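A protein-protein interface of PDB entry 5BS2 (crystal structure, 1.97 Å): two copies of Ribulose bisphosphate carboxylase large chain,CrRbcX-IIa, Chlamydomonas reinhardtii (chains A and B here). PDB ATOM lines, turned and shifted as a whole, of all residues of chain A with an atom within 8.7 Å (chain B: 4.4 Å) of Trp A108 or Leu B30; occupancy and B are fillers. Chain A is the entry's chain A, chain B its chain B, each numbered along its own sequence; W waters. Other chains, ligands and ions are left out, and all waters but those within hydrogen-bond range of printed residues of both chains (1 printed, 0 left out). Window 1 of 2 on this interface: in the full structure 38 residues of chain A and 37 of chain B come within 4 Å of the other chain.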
ATOM      1  N   PRO A  22     -13.437  -6.697 -18.258  1.00  0.00           N
ATOM      2  CA  PRO A  22     -12.523  -7.765 -17.838  1.00  0.00           C
ATOM      3  C   PRO A  22     -11.165  -7.211 -17.329  1.00  0.00           C
ATOM      4  O   PRO A  22     -10.623  -7.698 -16.351  1.00  0.00           O
ATOM      5  CB  PRO A  22     -12.354  -8.591 -19.103  1.00  0.00           C
ATOM      6  CG  PRO A  22     -13.635  -8.367 -19.868  1.00  0.00           C
ATOM      7  CD  PRO A  22     -14.042  -6.962 -19.573  1.00  0.00           C
ATOM      8  N   GLU A  23     -10.653  -6.200 -18.008  1.00  0.00           N
ATOM      9  CA  GLU A  23      -9.446  -5.497 -17.573  1.00  0.00           C
ATOM     10  C   GLU A  23      -9.585  -4.889 -16.175  1.00  0.00           C
ATOM     11  O   GLU A  23      -8.663  -4.920 -15.406  1.00  0.00           O
ATOM     12  CB  GLU A  23      -9.102  -4.396 -18.575  1.00  0.00           C
ATOM     13  CG  GLU A  23      -8.623  -4.900 -19.942  1.00  0.00           C
ATOM     14  CD  GLU A  23      -9.731  -5.175 -20.979  1.00  0.00           C
ATOM     15  OE1 GLU A  23     -10.949  -5.104 -20.644  1.00  0.00           O
ATOM     16  OE2 GLU A  23      -9.368  -5.437 -22.152  1.00  0.00           O
ATOM     17  N   LYS A  25     -11.839  -5.843 -13.718  1.00  0.00           N
ATOM     18  CA  LYS A  25     -11.843  -7.039 -12.866  1.00  0.00           C
ATOM     19  C   LYS A  25     -10.439  -7.548 -12.560  1.00  0.00           C
ATOM     20  O   LYS A  25     -10.090  -7.796 -11.413  1.00  0.00           O
ATOM     21  CB  LYS A  25     -12.624  -8.178 -13.527  1.00  0.00           C
ATOM     22  N   ALA A  26      -9.642  -7.709 -13.602  1.00  0.00           N
ATOM     23  CA  ALA A  26      -8.270  -8.158 -13.449  1.00  0.00           C
ATOM     24  C   ALA A  26      -7.437  -7.158 -12.653  1.00  0.00           C
ATOM     25  O   ALA A  26      -6.653  -7.555 -11.816  1.00  0.00           O
ATOM     26  CB  ALA A  26      -7.650  -8.430 -14.812  1.00  0.00           C
ATOM     27  N   ALA A  27      -7.614  -5.862 -12.897  1.00  0.00           N
ATOM     28  CA  ALA A  27      -6.868  -4.845 -12.163  1.00  0.00           C
ATOM     29  C   ALA A  27      -7.130  -4.887 -10.669  1.00  0.00           C
ATOM     30  O   ALA A  27      -6.200  -4.794  -9.841  1.00  0.00           O
ATOM     31  CB  ALA A  27      -7.206  -3.457 -12.670  1.00  0.00           C
ATOM     32  N   ALA A  29      -8.220  -7.330  -8.982  1.00  0.00           N
ATOM     33  CA  ALA A  29      -7.718  -8.570  -8.445  1.00  0.00           C
ATOM     34  C   ALA A  29      -6.192  -8.536  -8.241  1.00  0.00           C
ATOM     35  O   ALA A  29      -5.715  -8.977  -7.214  1.00  0.00           O
ATOM     36  CB  ALA A  29      -8.150  -9.756  -9.314  1.00  0.00           C
ATOM     37  N   LEU A  30      -5.464  -7.922  -9.178  1.00  0.00           N
ATOM     38  CA  LEU A  30      -4.049  -7.689  -9.027  1.00  0.00           C
ATOM     39  C   LEU A  30      -3.783  -6.851  -7.790  1.00  0.00           C
ATOM     40  O   LEU A  30      -2.900  -7.202  -6.982  1.00  0.00           O
ATOM     41  CB  LEU A  30      -3.454  -7.007 -10.266  1.00  0.00           C
ATOM     42  CG  LEU A  30      -3.325  -7.904 -11.501  1.00  0.00           C
ATOM     43  CD1 LEU A  30      -3.038  -7.093 -12.722  1.00  0.00           C
ATOM     44  CD2 LEU A  30      -2.232  -8.955 -11.320  1.00  0.00           C
ATOM     45  N   LEU A  33      -3.975  -8.913  -4.805  1.00  0.00           N
ATOM     46  CA  LEU A  33      -2.805  -9.827  -4.791  1.00  0.00           C
ATOM     47  C   LEU A  33      -1.591  -9.093  -4.223  1.00  0.00           C
ATOM     48  O   LEU A  33      -0.908  -9.602  -3.370  1.00  0.00           O
ATOM     49  CB  LEU A  33      -2.483 -10.318  -6.199  1.00  0.00           C
ATOM     50  CG  LEU A  33      -1.207 -11.140  -6.328  1.00  0.00           C
ATOM     51  CD1 LEU A  33      -1.320 -12.417  -5.502  1.00  0.00           C
ATOM     52  CD2 LEU A  33      -0.856 -11.430  -7.778  1.00  0.00           C
ATOM     53  N   PHE A  34      -1.408  -7.828  -4.636  1.00  0.00           N
ATOM     54  CA  PHE A  34      -0.278  -7.057  -4.151  1.00  0.00           C
ATOM     55  C   PHE A  34      -0.394  -6.750  -2.640  1.00  0.00           C
ATOM     56  O   PHE A  34       0.587  -6.825  -1.909  1.00  0.00           O
ATOM     57  CB  PHE A  34      -0.146  -5.745  -4.941  1.00  0.00           C
ATOM     58  CG  PHE A  34      -0.056  -5.919  -6.438  1.00  0.00           C
ATOM     59  CD1 PHE A  34       0.437  -7.069  -7.003  1.00  0.00           C
ATOM     60  CD2 PHE A  34      -0.461  -4.876  -7.291  1.00  0.00           C
ATOM     61  CE1 PHE A  34       0.519  -7.217  -8.370  1.00  0.00           C
ATOM     62  CE2 PHE A  34      -0.357  -5.005  -8.674  1.00  0.00           C
ATOM     63  CZ  PHE A  34       0.108  -6.196  -9.214  1.00  0.00           C
ATOM     64  N   TYR A 102       6.170  -3.252  -4.446  1.00  0.00           N
ATOM     65  CA  TYR A 102       5.962  -4.469  -5.218  1.00  0.00           C
ATOM     66  C   TYR A 102       5.505  -4.255  -6.673  1.00  0.00           C
ATOM     67  O   TYR A 102       5.807  -5.093  -7.547  1.00  0.00           O
ATOM     68  CB  TYR A 102       5.035  -5.422  -4.464  1.00  0.00           C
ATOM     69  CG  TYR A 102       4.994  -6.784  -5.062  1.00  0.00           C
ATOM     70  CD1 TYR A 102       3.804  -7.301  -5.553  1.00  0.00           C
ATOM     71  CD2 TYR A 102       6.140  -7.561  -5.144  1.00  0.00           C
ATOM     72  CE1 TYR A 102       3.756  -8.552  -6.129  1.00  0.00           C
ATOM     73  CE2 TYR A 102       6.112  -8.823  -5.722  1.00  0.00           C
ATOM     74  CZ  TYR A 102       4.891  -9.316  -6.196  1.00  0.00           C
ATOM     75  OH  TYR A 102       4.827 -10.547  -6.784  1.00  0.00           O
ATOM     76  N   LEU A 103       4.888  -3.088  -6.955  1.00  0.00           N
ATOM     77  CA  LEU A 103       4.533  -2.684  -8.330  1.00  0.00           C
ATOM     78  C   LEU A 103       5.749  -2.620  -9.248  1.00  0.00           C
ATOM     79  O   LEU A 103       5.620  -2.768 -10.461  1.00  0.00           O
ATOM     80  CB  LEU A 103       3.911  -1.269  -8.354  1.00  0.00           C
ATOM     81  CG  LEU A 103       2.673  -0.977  -7.540  1.00  0.00           C
ATOM     82  CD1 LEU A 103       2.284   0.491  -7.676  1.00  0.00           C
ATOM     83  CD2 LEU A 103       1.546  -1.896  -7.996  1.00  0.00           C
ATOM     84  N   ASP A 104       6.916  -2.333  -8.680  1.00  0.00           N
ATOM     85  CA  ASP A 104       8.167  -2.268  -9.442  1.00  0.00           C
ATOM     86  C   ASP A 104       8.850  -3.629  -9.642  1.00  0.00           C
ATOM     87  O   ASP A 104       9.770  -3.709 -10.461  1.00  0.00           O
ATOM     88  CB  ASP A 104       9.177  -1.314  -8.792  1.00  0.00           C
ATOM     89  CG  ASP A 104       8.609   0.092  -8.543  1.00  0.00           C
ATOM     90  OD1 ASP A 104       7.646   0.485  -9.250  1.00  0.00           O
ATOM     91  OD2 ASP A 104       9.118   0.798  -7.625  1.00  0.00           O
ATOM     92  N   GLU A 105       8.391  -4.678  -8.938  1.00  0.00           N
ATOM     93  CA  GLU A 105       9.018  -6.012  -8.930  1.00  0.00           C
ATOM     94  C   GLU A 105       8.185  -7.106  -9.582  1.00  0.00           C
ATOM     95  O   GLU A 105       8.726  -8.000 -10.226  1.00  0.00           O
ATOM     96  CB  GLU A 105       9.326  -6.444  -7.494  1.00  0.00           C
ATOM     97  CG  GLU A 105      10.350  -5.503  -6.838  1.00  0.00           C
ATOM     98  CD  GLU A 105      10.383  -5.551  -5.317  1.00  0.00           C
ATOM     99  OE1 GLU A 105       9.340  -5.906  -4.676  1.00  0.00           O
ATOM    100  OE2 GLU A 105      11.450  -5.193  -4.767  1.00  0.00           O
ATOM    101  N   PHE A 106       6.862  -7.043  -9.383  1.00  0.00           N
ATOM    102  CA  PHE A 106       5.934  -7.924 -10.051  1.00  0.00           C
ATOM    103  C   PHE A 106       6.188  -8.006 -11.538  1.00  0.00           C
ATOM    104  O   PHE A 106       6.280  -6.986 -12.250  1.00  0.00           O
ATOM    105  CB  PHE A 106       4.515  -7.424  -9.804  1.00  0.00           C
ATOM    106  CG  PHE A 106       3.467  -8.328 -10.335  1.00  0.00           C
ATOM    107  CD1 PHE A 106       3.324  -9.604  -9.805  1.00  0.00           C
ATOM    108  CD2 PHE A 106       2.674  -7.938 -11.388  1.00  0.00           C
ATOM    109  CE1 PHE A 106       2.362 -10.449 -10.283  1.00  0.00           C
ATOM    110  CE2 PHE A 106       1.706  -8.781 -11.880  1.00  0.00           C
ATOM    111  CZ  PHE A 106       1.537 -10.033 -11.322  1.00  0.00           C
ATOM    112  N   GLU A 107       6.342  -9.227 -12.015  1.00  0.00           N
ATOM    113  CA  GLU A 107       6.748  -9.468 -13.396  1.00  0.00           C
ATOM    114  C   GLU A 107       5.477  -9.692 -14.242  1.00  0.00           C
ATOM    115  O   GLU A 107       5.048 -10.810 -14.460  1.00  0.00           O
ATOM    116  CB  GLU A 107       7.741 -10.641 -13.465  1.00  0.00           C
ATOM    117  CG  GLU A 107       9.047 -10.284 -12.755  1.00  0.00           C
ATOM    118  CD  GLU A 107      10.068 -11.412 -12.729  1.00  0.00           C
ATOM    119  OE1 GLU A 107      10.014 -12.317 -13.581  1.00  0.00           O
ATOM    120  OE2 GLU A 107      10.952 -11.379 -11.865  1.00  0.00           O
ATOM    121  N   TRP A 108       4.888  -8.571 -14.676  1.00  0.00           N
ATOM    122  CA  TRP A 108       3.679  -8.565 -15.474  1.00  0.00           C
ATOM    123  C   TRP A 108       3.909  -9.189 -16.843  1.00  0.00           C
ATOM    124  O   TRP A 108       3.039  -9.872 -17.358  1.00  0.00           O
ATOM    125  CB  TRP A 108       3.126  -7.165 -15.614  1.00  0.00           C
ATOM    126  CG  TRP A 108       1.843  -7.025 -16.460  1.00  0.00           C
ATOM    127  CD1 TRP A 108       1.659  -6.154 -17.497  1.00  0.00           C
ATOM    128  CD2 TRP A 108       0.594  -7.688 -16.283  1.00  0.00           C
ATOM    129  NE1 TRP A 108       0.402  -6.256 -18.004  1.00  0.00           N
ATOM    130  CE2 TRP A 108      -0.282  -7.191 -17.273  1.00  0.00           C
ATOM    131  CE3 TRP A 108       0.130  -8.682 -15.415  1.00  0.00           C
ATOM    132  CZ2 TRP A 108      -1.601  -7.638 -17.403  1.00  0.00           C
ATOM    133  CZ3 TRP A 108      -1.205  -9.108 -15.539  1.00  0.00           C
ATOM    134  CH2 TRP A 108      -2.040  -8.585 -16.529  1.00  0.00           C
ATOM    135  N   GLY A 109       5.073  -8.969 -17.423  1.00  0.00           N
ATOM    136  CA  GLY A 109       5.422  -9.575 -18.695  1.00  0.00           C
ATOM    137  C   GLY A 109       5.383 -11.083 -18.618  1.00  0.00           C
ATOM    138  O   GLY A 109       4.794 -11.743 -19.473  1.00  0.00           O
ATOM    139  N   LYS A 110       6.031 -11.631 -17.601  1.00  0.00           N
ATOM    140  CA  LYS A 110       6.063 -13.067 -17.399  1.00  0.00           C
ATOM    141  C   LYS A 110       4.648 -13.599 -17.239  1.00  0.00           C
ATOM    142  O   LYS A 110       4.295 -14.607 -17.814  1.00  0.00           O
ATOM    143  CB  LYS A 110       6.914 -13.412 -16.168  1.00  0.00           C
ATOM    144  CG  LYS A 110       6.891 -14.885 -15.786  1.00  0.00           C
ATOM    145  CD  LYS A 110       7.668 -15.157 -14.506  1.00  0.00           C
ATOM    146  CE  LYS A 110       9.132 -15.351 -14.803  1.00  0.00           C
ATOM    147  NZ  LYS A 110       9.868 -15.841 -13.601  1.00  0.00           N
ATOM    148  N   THR A 111       3.846 -12.891 -16.450  1.00  0.00           N
ATOM    149  CA  THR A 111       2.467 -13.245 -16.201  1.00  0.00           C
ATOM    150  C   THR A 111       1.670 -13.347 -17.510  1.00  0.00           C
ATOM    151  O   THR A 111       0.999 -14.331 -17.798  1.00  0.00           O
ATOM    152  CB  THR A 111       1.797 -12.183 -15.270  1.00  0.00           C
ATOM    153  OG1 THR A 111       2.424 -12.185 -13.984  1.00  0.00           O
ATOM    154  CG2 THR A 111       0.361 -12.419 -15.095  1.00  0.00           C
ATOM    155  N   MET A 112       1.751 -12.288 -18.288  1.00  0.00           N
ATOM    156  CA  MET A 112       1.065 -12.160 -19.532  1.00  0.00           C
ATOM    157  C   MET A 112       1.551 -13.236 -20.506  1.00  0.00           C
ATOM    158  O   MET A 112       0.749 -13.937 -21.175  1.00  0.00           O
ATOM    159  CB  MET A 112       1.305 -10.688 -19.930  1.00  0.00           C
ATOM    160  CG  MET A 112       1.204 -10.216 -21.335  1.00  0.00           C
ATOM    161  SD  MET A 112       1.393  -8.373 -21.317  1.00  0.00           S
ATOM    162  CE  MET A 112       0.821  -8.144 -22.998  1.00  0.00           C
ATOM    163  N   GLU A 113       2.850 -13.462 -20.503  1.00  0.00           N
ATOM    164  CA  GLU A 113       3.436 -14.519 -21.292  1.00  0.00           C
ATOM    165  C   GLU A 113       2.890 -15.919 -20.969  1.00  0.00           C
ATOM    166  O   GLU A 113       2.582 -16.682 -21.861  1.00  0.00           O
ATOM    167  CB  GLU A 113       4.952 -14.547 -21.083  1.00  0.00           C
ATOM    168  CG  GLU A 113       5.602 -15.762 -21.753  1.00  0.00           C
ATOM    169  CD  GLU A 113       5.342 -15.799 -23.239  1.00  0.00           C
ATOM    170  OE1 GLU A 113       4.892 -14.753 -23.777  1.00  0.00           O
ATOM    171  OE2 GLU A 113       5.576 -16.864 -23.875  1.00  0.00           O
ATOM    172  N   MET A 114       2.887 -16.259 -19.690  1.00  0.00           N
ATOM    173  CA  MET A 114       2.373 -17.532 -19.216  1.00  0.00           C
ATOM    174  C   MET A 114       0.893 -17.686 -19.531  1.00  0.00           C
ATOM    175  O   MET A 114       0.457 -18.746 -19.960  1.00  0.00           O
ATOM    176  CB  MET A 114       2.584 -17.686 -17.711  1.00  0.00           C
ATOM    177  CG  MET A 114       4.031 -17.865 -17.281  1.00  0.00           C
ATOM    178  SD  MET A 114       4.172 -18.317 -15.536  1.00  0.00           S
ATOM    179  CE  MET A 114       3.649 -16.833 -14.716  1.00  0.00           C
ATOM    180  N   ALA A 115       0.110 -16.632 -19.296  1.00  0.00           N
ATOM    181  CA  ALA A 115      -1.320 -16.713 -19.559  1.00  0.00           C
ATOM    182  C   ALA A 115      -1.553 -17.000 -21.037  1.00  0.00           C
ATOM    183  O   ALA A 115      -2.377 -17.837 -21.374  1.00  0.00           O
ATOM    184  CB  ALA A 115      -2.040 -15.457 -19.128  1.00  0.00           C
ATOM    185  N   SER A 116      -0.776 -16.373 -21.919  1.00  0.00           N
ATOM    186  CA  SER A 116      -0.941 -16.564 -23.369  1.00  0.00           C
ATOM    187  C   SER A 116      -0.473 -17.913 -23.863  1.00  0.00           C
ATOM    188  O   SER A 116      -1.195 -18.580 -24.562  1.00  0.00           O
ATOM    189  CB  SER A 116      -0.172 -15.505 -24.154  1.00  0.00           C
ATOM    190  OG  SER A 116      -0.608 -14.233 -23.748  1.00  0.00           O
ATOM    191  N   THR A 119      -2.665 -20.800 -22.633  1.00  0.00           N
ATOM    192  CA  THR A 119      -3.899 -20.800 -23.378  1.00  0.00           C
ATOM    193  C   THR A 119      -3.754 -21.535 -24.716  1.00  0.00           C
ATOM    194  O   THR A 119      -4.542 -22.427 -25.037  1.00  0.00           O
ATOM    195  CB  THR A 119      -4.465 -19.373 -23.569  1.00  0.00           C
ATOM    196  OG1 THR A 119      -4.862 -18.844 -22.293  1.00  0.00           O
ATOM    197  CG2 THR A 119      -5.693 -19.375 -24.534  1.00  0.00           C
ATOM    198  N   ALA B  26      -1.629 -15.166 -10.747  1.00  0.00           N
ATOM    199  CA  ALA B  26      -2.274 -14.204 -11.578  1.00  0.00           C
ATOM    200  C   ALA B  26      -2.506 -14.778 -12.976  1.00  0.00           C
ATOM    201  O   ALA B  26      -3.549 -14.522 -13.557  1.00  0.00           O
ATOM    202  CB  ALA B  26      -1.422 -12.924 -11.647  1.00  0.00           C
ATOM    203  N   ALA B  27      -1.563 -15.565 -13.496  1.00  0.00           N
ATOM    204  CA  ALA B  27      -1.690 -16.095 -14.868  1.00  0.00           C
ATOM    205  C   ALA B  27      -2.875 -17.040 -15.002  1.00  0.00           C
ATOM    206  O   ALA B  27      -3.634 -16.979 -15.940  1.00  0.00           O
ATOM    207  CB  ALA B  27      -0.434 -16.814 -15.289  1.00  0.00           C
ATOM    208  N   VAL B  28      -2.964 -17.933 -14.037  1.00  0.00           N
ATOM    209  CA  VAL B  28      -3.979 -18.943 -14.051  1.00  0.00           C
ATOM    210  C   VAL B  28      -5.343 -18.273 -13.887  1.00  0.00           C
ATOM    211  O   VAL B  28      -6.279 -18.617 -14.583  1.00  0.00           O
ATOM    212  CB  VAL B  28      -3.710 -20.000 -12.974  1.00  0.00           C
ATOM    213  CG1 VAL B  28      -4.838 -21.045 -12.968  1.00  0.00           C
ATOM    214  CG2 VAL B  28      -2.386 -20.693 -13.249  1.00  0.00           C
ATOM    215  N   ALA B  29      -5.419 -17.238 -13.051  1.00  0.00           N
ATOM    216  CA  ALA B  29      -6.665 -16.495 -12.866  1.00  0.00           C
ATOM    217  C   ALA B  29      -7.083 -15.767 -14.143  1.00  0.00           C
ATOM    218  O   ALA B  29      -8.262 -15.778 -14.505  1.00  0.00           O
ATOM    219  CB  ALA B  29      -6.562 -15.533 -11.679  1.00  0.00           C
ATOM    220  N   LEU B  30      -6.123 -15.162 -14.844  1.00  0.00           N
ATOM    221  CA  LEU B  30      -6.402 -14.526 -16.121  1.00  0.00           C
ATOM    222  C   LEU B  30      -6.933 -15.546 -17.107  1.00  0.00           C
ATOM    223  O   LEU B  30      -7.925 -15.260 -17.807  1.00  0.00           O
ATOM    224  CB  LEU B  30      -5.154 -13.858 -16.700  1.00  0.00           C
ATOM    225  CG  LEU B  30      -4.712 -12.559 -16.023  1.00  0.00           C
ATOM    226  CD1 LEU B  30      -3.303 -12.204 -16.464  1.00  0.00           C
ATOM    227  CD2 LEU B  30      -5.663 -11.397 -16.326  1.00  0.00           C
ATOM    228  N   ARG B  31      -6.302 -16.722 -17.150  1.00  0.00           N
ATOM    229  CA  ARG B  31      -6.733 -17.756 -18.073  1.00  0.00           C
ATOM    230  C   ARG B  31      -8.212 -18.131 -17.833  1.00  0.00           C
ATOM    231  O   ARG B  31      -8.962 -18.312 -18.763  1.00  0.00           O
ATOM    232  CB  ARG B  31      -5.837 -19.012 -17.986  1.00  0.00           C
ATOM    233  CG  ARG B  31      -4.437 -18.788 -18.605  1.00  0.00           C
ATOM    234  CD  ARG B  31      -3.773 -20.057 -19.036  1.00  0.00           C
ATOM    235  NE  ARG B  31      -4.718 -20.708 -19.913  1.00  0.00           N
ATOM    236  CZ  ARG B  31      -5.135 -21.964 -19.824  1.00  0.00           C
ATOM    237  NH1 ARG B  31      -6.131 -22.353 -20.643  1.00  0.00           N
ATOM    238  NH2 ARG B  31      -4.602 -22.794 -18.929  1.00  0.00           N
ATOM    239  N   SER B  32      -8.621 -18.191 -16.584  1.00  0.00           N
ATOM    240  CA  SER B  32     -10.043 -18.445 -16.285  1.00  0.00           C
ATOM    241  C   SER B  32     -10.927 -17.246 -16.701  1.00  0.00           C
ATOM    242  O   SER B  32     -12.025 -17.408 -17.240  1.00  0.00           O
ATOM    243  CB  SER B  32     -10.229 -18.764 -14.816  1.00  0.00           C
ATOM    244  OG  SER B  32      -9.435 -19.882 -14.450  1.00  0.00           O
ATOM    245  N   LEU B  33     -10.425 -16.040 -16.518  1.00  0.00           N
ATOM    246  CA  LEU B  33     -11.178 -14.885 -16.965  1.00  0.00           C
ATOM    247  C   LEU B  33     -11.440 -14.997 -18.461  1.00  0.00           C
ATOM    248  O   LEU B  33     -12.546 -14.694 -18.944  1.00  0.00           O
ATOM    249  CB  LEU B  33     -10.417 -13.587 -16.636  1.00  0.00           C
ATOM    250  CG  LEU B  33     -11.047 -12.308 -17.137  1.00  0.00           C
ATOM    251  CD1 LEU B  33     -12.431 -12.097 -16.549  1.00  0.00           C
ATOM    252  CD2 LEU B  33     -10.155 -11.084 -16.872  1.00  0.00           C
ATOM    253  N   PHE B  34     -10.407 -15.329 -19.227  1.00  0.00           N
ATOM    254  CA  PHE B  34     -10.508 -15.360 -20.684  1.00  0.00           C
ATOM    255  C   PHE B  34     -11.487 -16.457 -21.137  1.00  0.00           C
ATOM    256  O   PHE B  34     -12.270 -16.284 -22.063  1.00  0.00           O
ATOM    257  CB  PHE B  34      -9.141 -15.608 -21.323  1.00  0.00           C
ATOM    258  CG  PHE B  34      -8.065 -14.571 -20.963  1.00  0.00           C
ATOM    259  CD1 PHE B  34      -8.401 -13.277 -20.542  1.00  0.00           C
ATOM    260  CD2 PHE B  34      -6.714 -14.895 -21.036  1.00  0.00           C
ATOM    261  CE1 PHE B  34      -7.424 -12.351 -20.214  1.00  0.00           C
ATOM    262  CE2 PHE B  34      -5.722 -13.945 -20.741  1.00  0.00           C
ATOM    263  CZ  PHE B  34      -6.076 -12.684 -20.325  1.00  0.00           C
ATOM    264  N   PHE B 106      -7.645  -8.236 -25.153  1.00  0.00           N
ATOM    265  CA  PHE B 106      -7.437  -7.843 -23.791  1.00  0.00           C
ATOM    266  C   PHE B 106      -6.334  -6.793 -23.677  1.00  0.00           C
ATOM    267  O   PHE B 106      -5.216  -6.982 -24.185  1.00  0.00           O
ATOM    268  CB  PHE B 106      -7.058  -9.058 -22.987  1.00  0.00           C
ATOM    269  CG  PHE B 106      -7.015  -8.811 -21.511  1.00  0.00           C
ATOM    270  CD1 PHE B 106      -8.174  -8.504 -20.807  1.00  0.00           C
ATOM    271  CD2 PHE B 106      -5.815  -8.923 -20.819  1.00  0.00           C
ATOM    272  CE1 PHE B 106      -8.124  -8.303 -19.436  1.00  0.00           C
ATOM    273  CE2 PHE B 106      -5.755  -8.708 -19.453  1.00  0.00           C
ATOM    274  CZ  PHE B 106      -6.916  -8.424 -18.760  1.00  0.00           C
ATOM    275  N   TRP B 108      -3.790  -5.534 -21.784  1.00  0.00           N
ATOM    276  CA  TRP B 108      -2.862  -5.883 -20.722  1.00  0.00           C
ATOM    277  C   TRP B 108      -2.150  -4.671 -20.138  1.00  0.00           C
ATOM    278  O   TRP B 108      -1.957  -4.557 -18.933  1.00  0.00           O
ATOM    279  CB  TRP B 108      -1.795  -6.816 -21.322  1.00  0.00           C
ATOM    280  CG  TRP B 108      -2.326  -8.054 -22.034  1.00  0.00           C
ATOM    281  CD1 TRP B 108      -2.790  -8.162 -23.336  1.00  0.00           C
ATOM    282  CD2 TRP B 108      -2.413  -9.363 -21.476  1.00  0.00           C
ATOM    283  NE1 TRP B 108      -3.167  -9.470 -23.598  1.00  0.00           N
ATOM    284  CE2 TRP B 108      -2.935 -10.224 -22.479  1.00  0.00           C
ATOM    285  CE3 TRP B 108      -2.064  -9.904 -20.236  1.00  0.00           C
ATOM    286  CZ2 TRP B 108      -3.117 -11.579 -22.266  1.00  0.00           C
ATOM    287  CZ3 TRP B 108      -2.275 -11.242 -20.022  1.00  0.00           C
ATOM    288  CH2 TRP B 108      -2.806 -12.068 -21.025  1.00  0.00           C
ATOM    289  N   THR B 111      -4.553  -2.690 -18.009  1.00  0.00           N
ATOM    290  CA  THR B 111      -4.746  -3.485 -16.807  1.00  0.00           C
ATOM    291  C   THR B 111      -3.669  -3.248 -15.762  1.00  0.00           C
ATOM    292  O   THR B 111      -3.951  -2.900 -14.592  1.00  0.00           O
ATOM    293  CB  THR B 111      -4.781  -4.985 -17.172  1.00  0.00           C
ATOM    294  OG1 THR B 111      -5.904  -5.256 -17.998  1.00  0.00           O
ATOM    295  CG2 THR B 111      -4.885  -5.841 -15.945  1.00  0.00           C
ATOM    296  N   MET B 112      -2.425  -3.420 -16.171  1.00  0.00           N
ATOM    297  CA  MET B 112      -1.316  -3.190 -15.224  1.00  0.00           C
ATOM    298  C   MET B 112      -1.262  -1.704 -14.820  1.00  0.00           C
ATOM    299  O   MET B 112      -1.050  -1.369 -13.667  1.00  0.00           O
ATOM    300  CB  MET B 112       0.047  -3.698 -15.735  1.00  0.00           C
ATOM    301  CG  MET B 112       1.111  -3.804 -14.624  1.00  0.00           C
ATOM    302  SD  MET B 112       0.601  -4.869 -13.227  1.00  0.00           S
ATOM    303  CE  MET B 112       1.815  -4.308 -12.038  1.00  0.00           C
HETATM  304  O   HOH W   1      -7.601 -19.747 -21.072  1.00  0.00           O
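NE1 of Trp A108 lies within hydrogen-bond range of O of Trp B108 (3.1 Å). OG1 of Thr A119 sits at hydrogen-bond distance from NE of Arg B31, 3.0 Å away.
OG1 of Thr A111 is in hydrogen-bond range of O of Glu A107, at 3.0 Å. The side-chain hydroxyl (OG) of Ser A116 sits at hydrogen-bond distance from the backbone carbonyl oxygen (O) of Met A112 (2.9 Å). The backbone carbonyl oxygen (O) of Ala A115 lies within hydrogen-bond range of the side-chain hydroxyl (OG1) of Thr A119. The backbone carbonyl oxygen (O) of Phe B106 sits close to the indole nitrogen (NE1) of Trp B108, at 3.3 Å.
Glu A23 touches Phe B106. Thr B111 touches Glu A23. Ala A26 touches Leu B30 (CB to CD2, 3.9 Å). Thr B111 touches Leu A30 (CG2 to CD1, 3.9 Å). Met B112 touches Phe A106. CD1 of Leu B30 touches CH2 of Trp A108, 3.8 Å away. CG2 of Thr A111 touches CD1 of Leu B30, 3.9 Å away. Ala A115 touches Arg B31. CB of Ala A115 touches CH2 of Trp B108, at 3.96 Å. CZ2 of Trp B108 touches OG of Ser A116, at 3.9 Å.
Of the printed residues of chain B, Pro A22 touches Leu B33 and Phe B106. Asp A104 touches none of the printed residues of chain B. Of the printed residues of chain B, Trp A108 touches Leu B30 (3.8 Å), Trp B108 (3.1 Å), Thr B111 (3.996 Å) and Met B112 (3.4 Å). Of the printed residues of chain A, Ala B26 touches Thr A111 (3.9 Å). Printed residues of chain A within 4 Å of Leu B30: Ala A26, Trp A108 and Thr A111. Of the printed residues of chain A, Trp B108 touches Trp A108 (3.1 Å), Met A112 (3.3 Å), Ala A115 (3.96 Å) and Ser A116 (3.9 Å). Of the printed residues of chain A, Met B112 touches Phe A34 (3.8 Å), Phe A106 (3.8 Å) and Trp A108 (3.4 Å).
Of the 25 printed residues of chain A, 14 touch a printed residue of chain B. Hydrophobic or aromatic side chains of chain A that line the printed part of chain B: Ala A26, Ala A27, Leu A30, Phe A34, Phe A106, Trp A108, Met A112, Met A114 and Ala A115. Hydrophobic or aromatic side chains of chain B that line the printed part of chain A: Ala B26, Ala B27, Leu B30, Leu B33, Phe B106, Trp B108 and Met B112. Among the printed residues, 24 pairs touch across the chains.
Ala A26 touches Leu B30, but with the chains exchanged Leu A30 does not touch Ala B26 (4.1 Å). Phe A106 touches Met B112, but with the chains exchanged Met A112 does not touch Phe B106 (6.3 Å). Trp A108 touches its own counterpart, Trp B108. Trp A108 touches Thr B111, but with the chains exchanged Thr A111 does not touch Trp B108 (5.0 Å). Of the 24 pairs that touch across the chains among the printed residues, 9 have their exchanged pair printed and touching as well.
Water W1 lies within hydrogen-bond range of the guanidinium group of Arg B31 and the side-chain hydroxyl of Thr A119.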
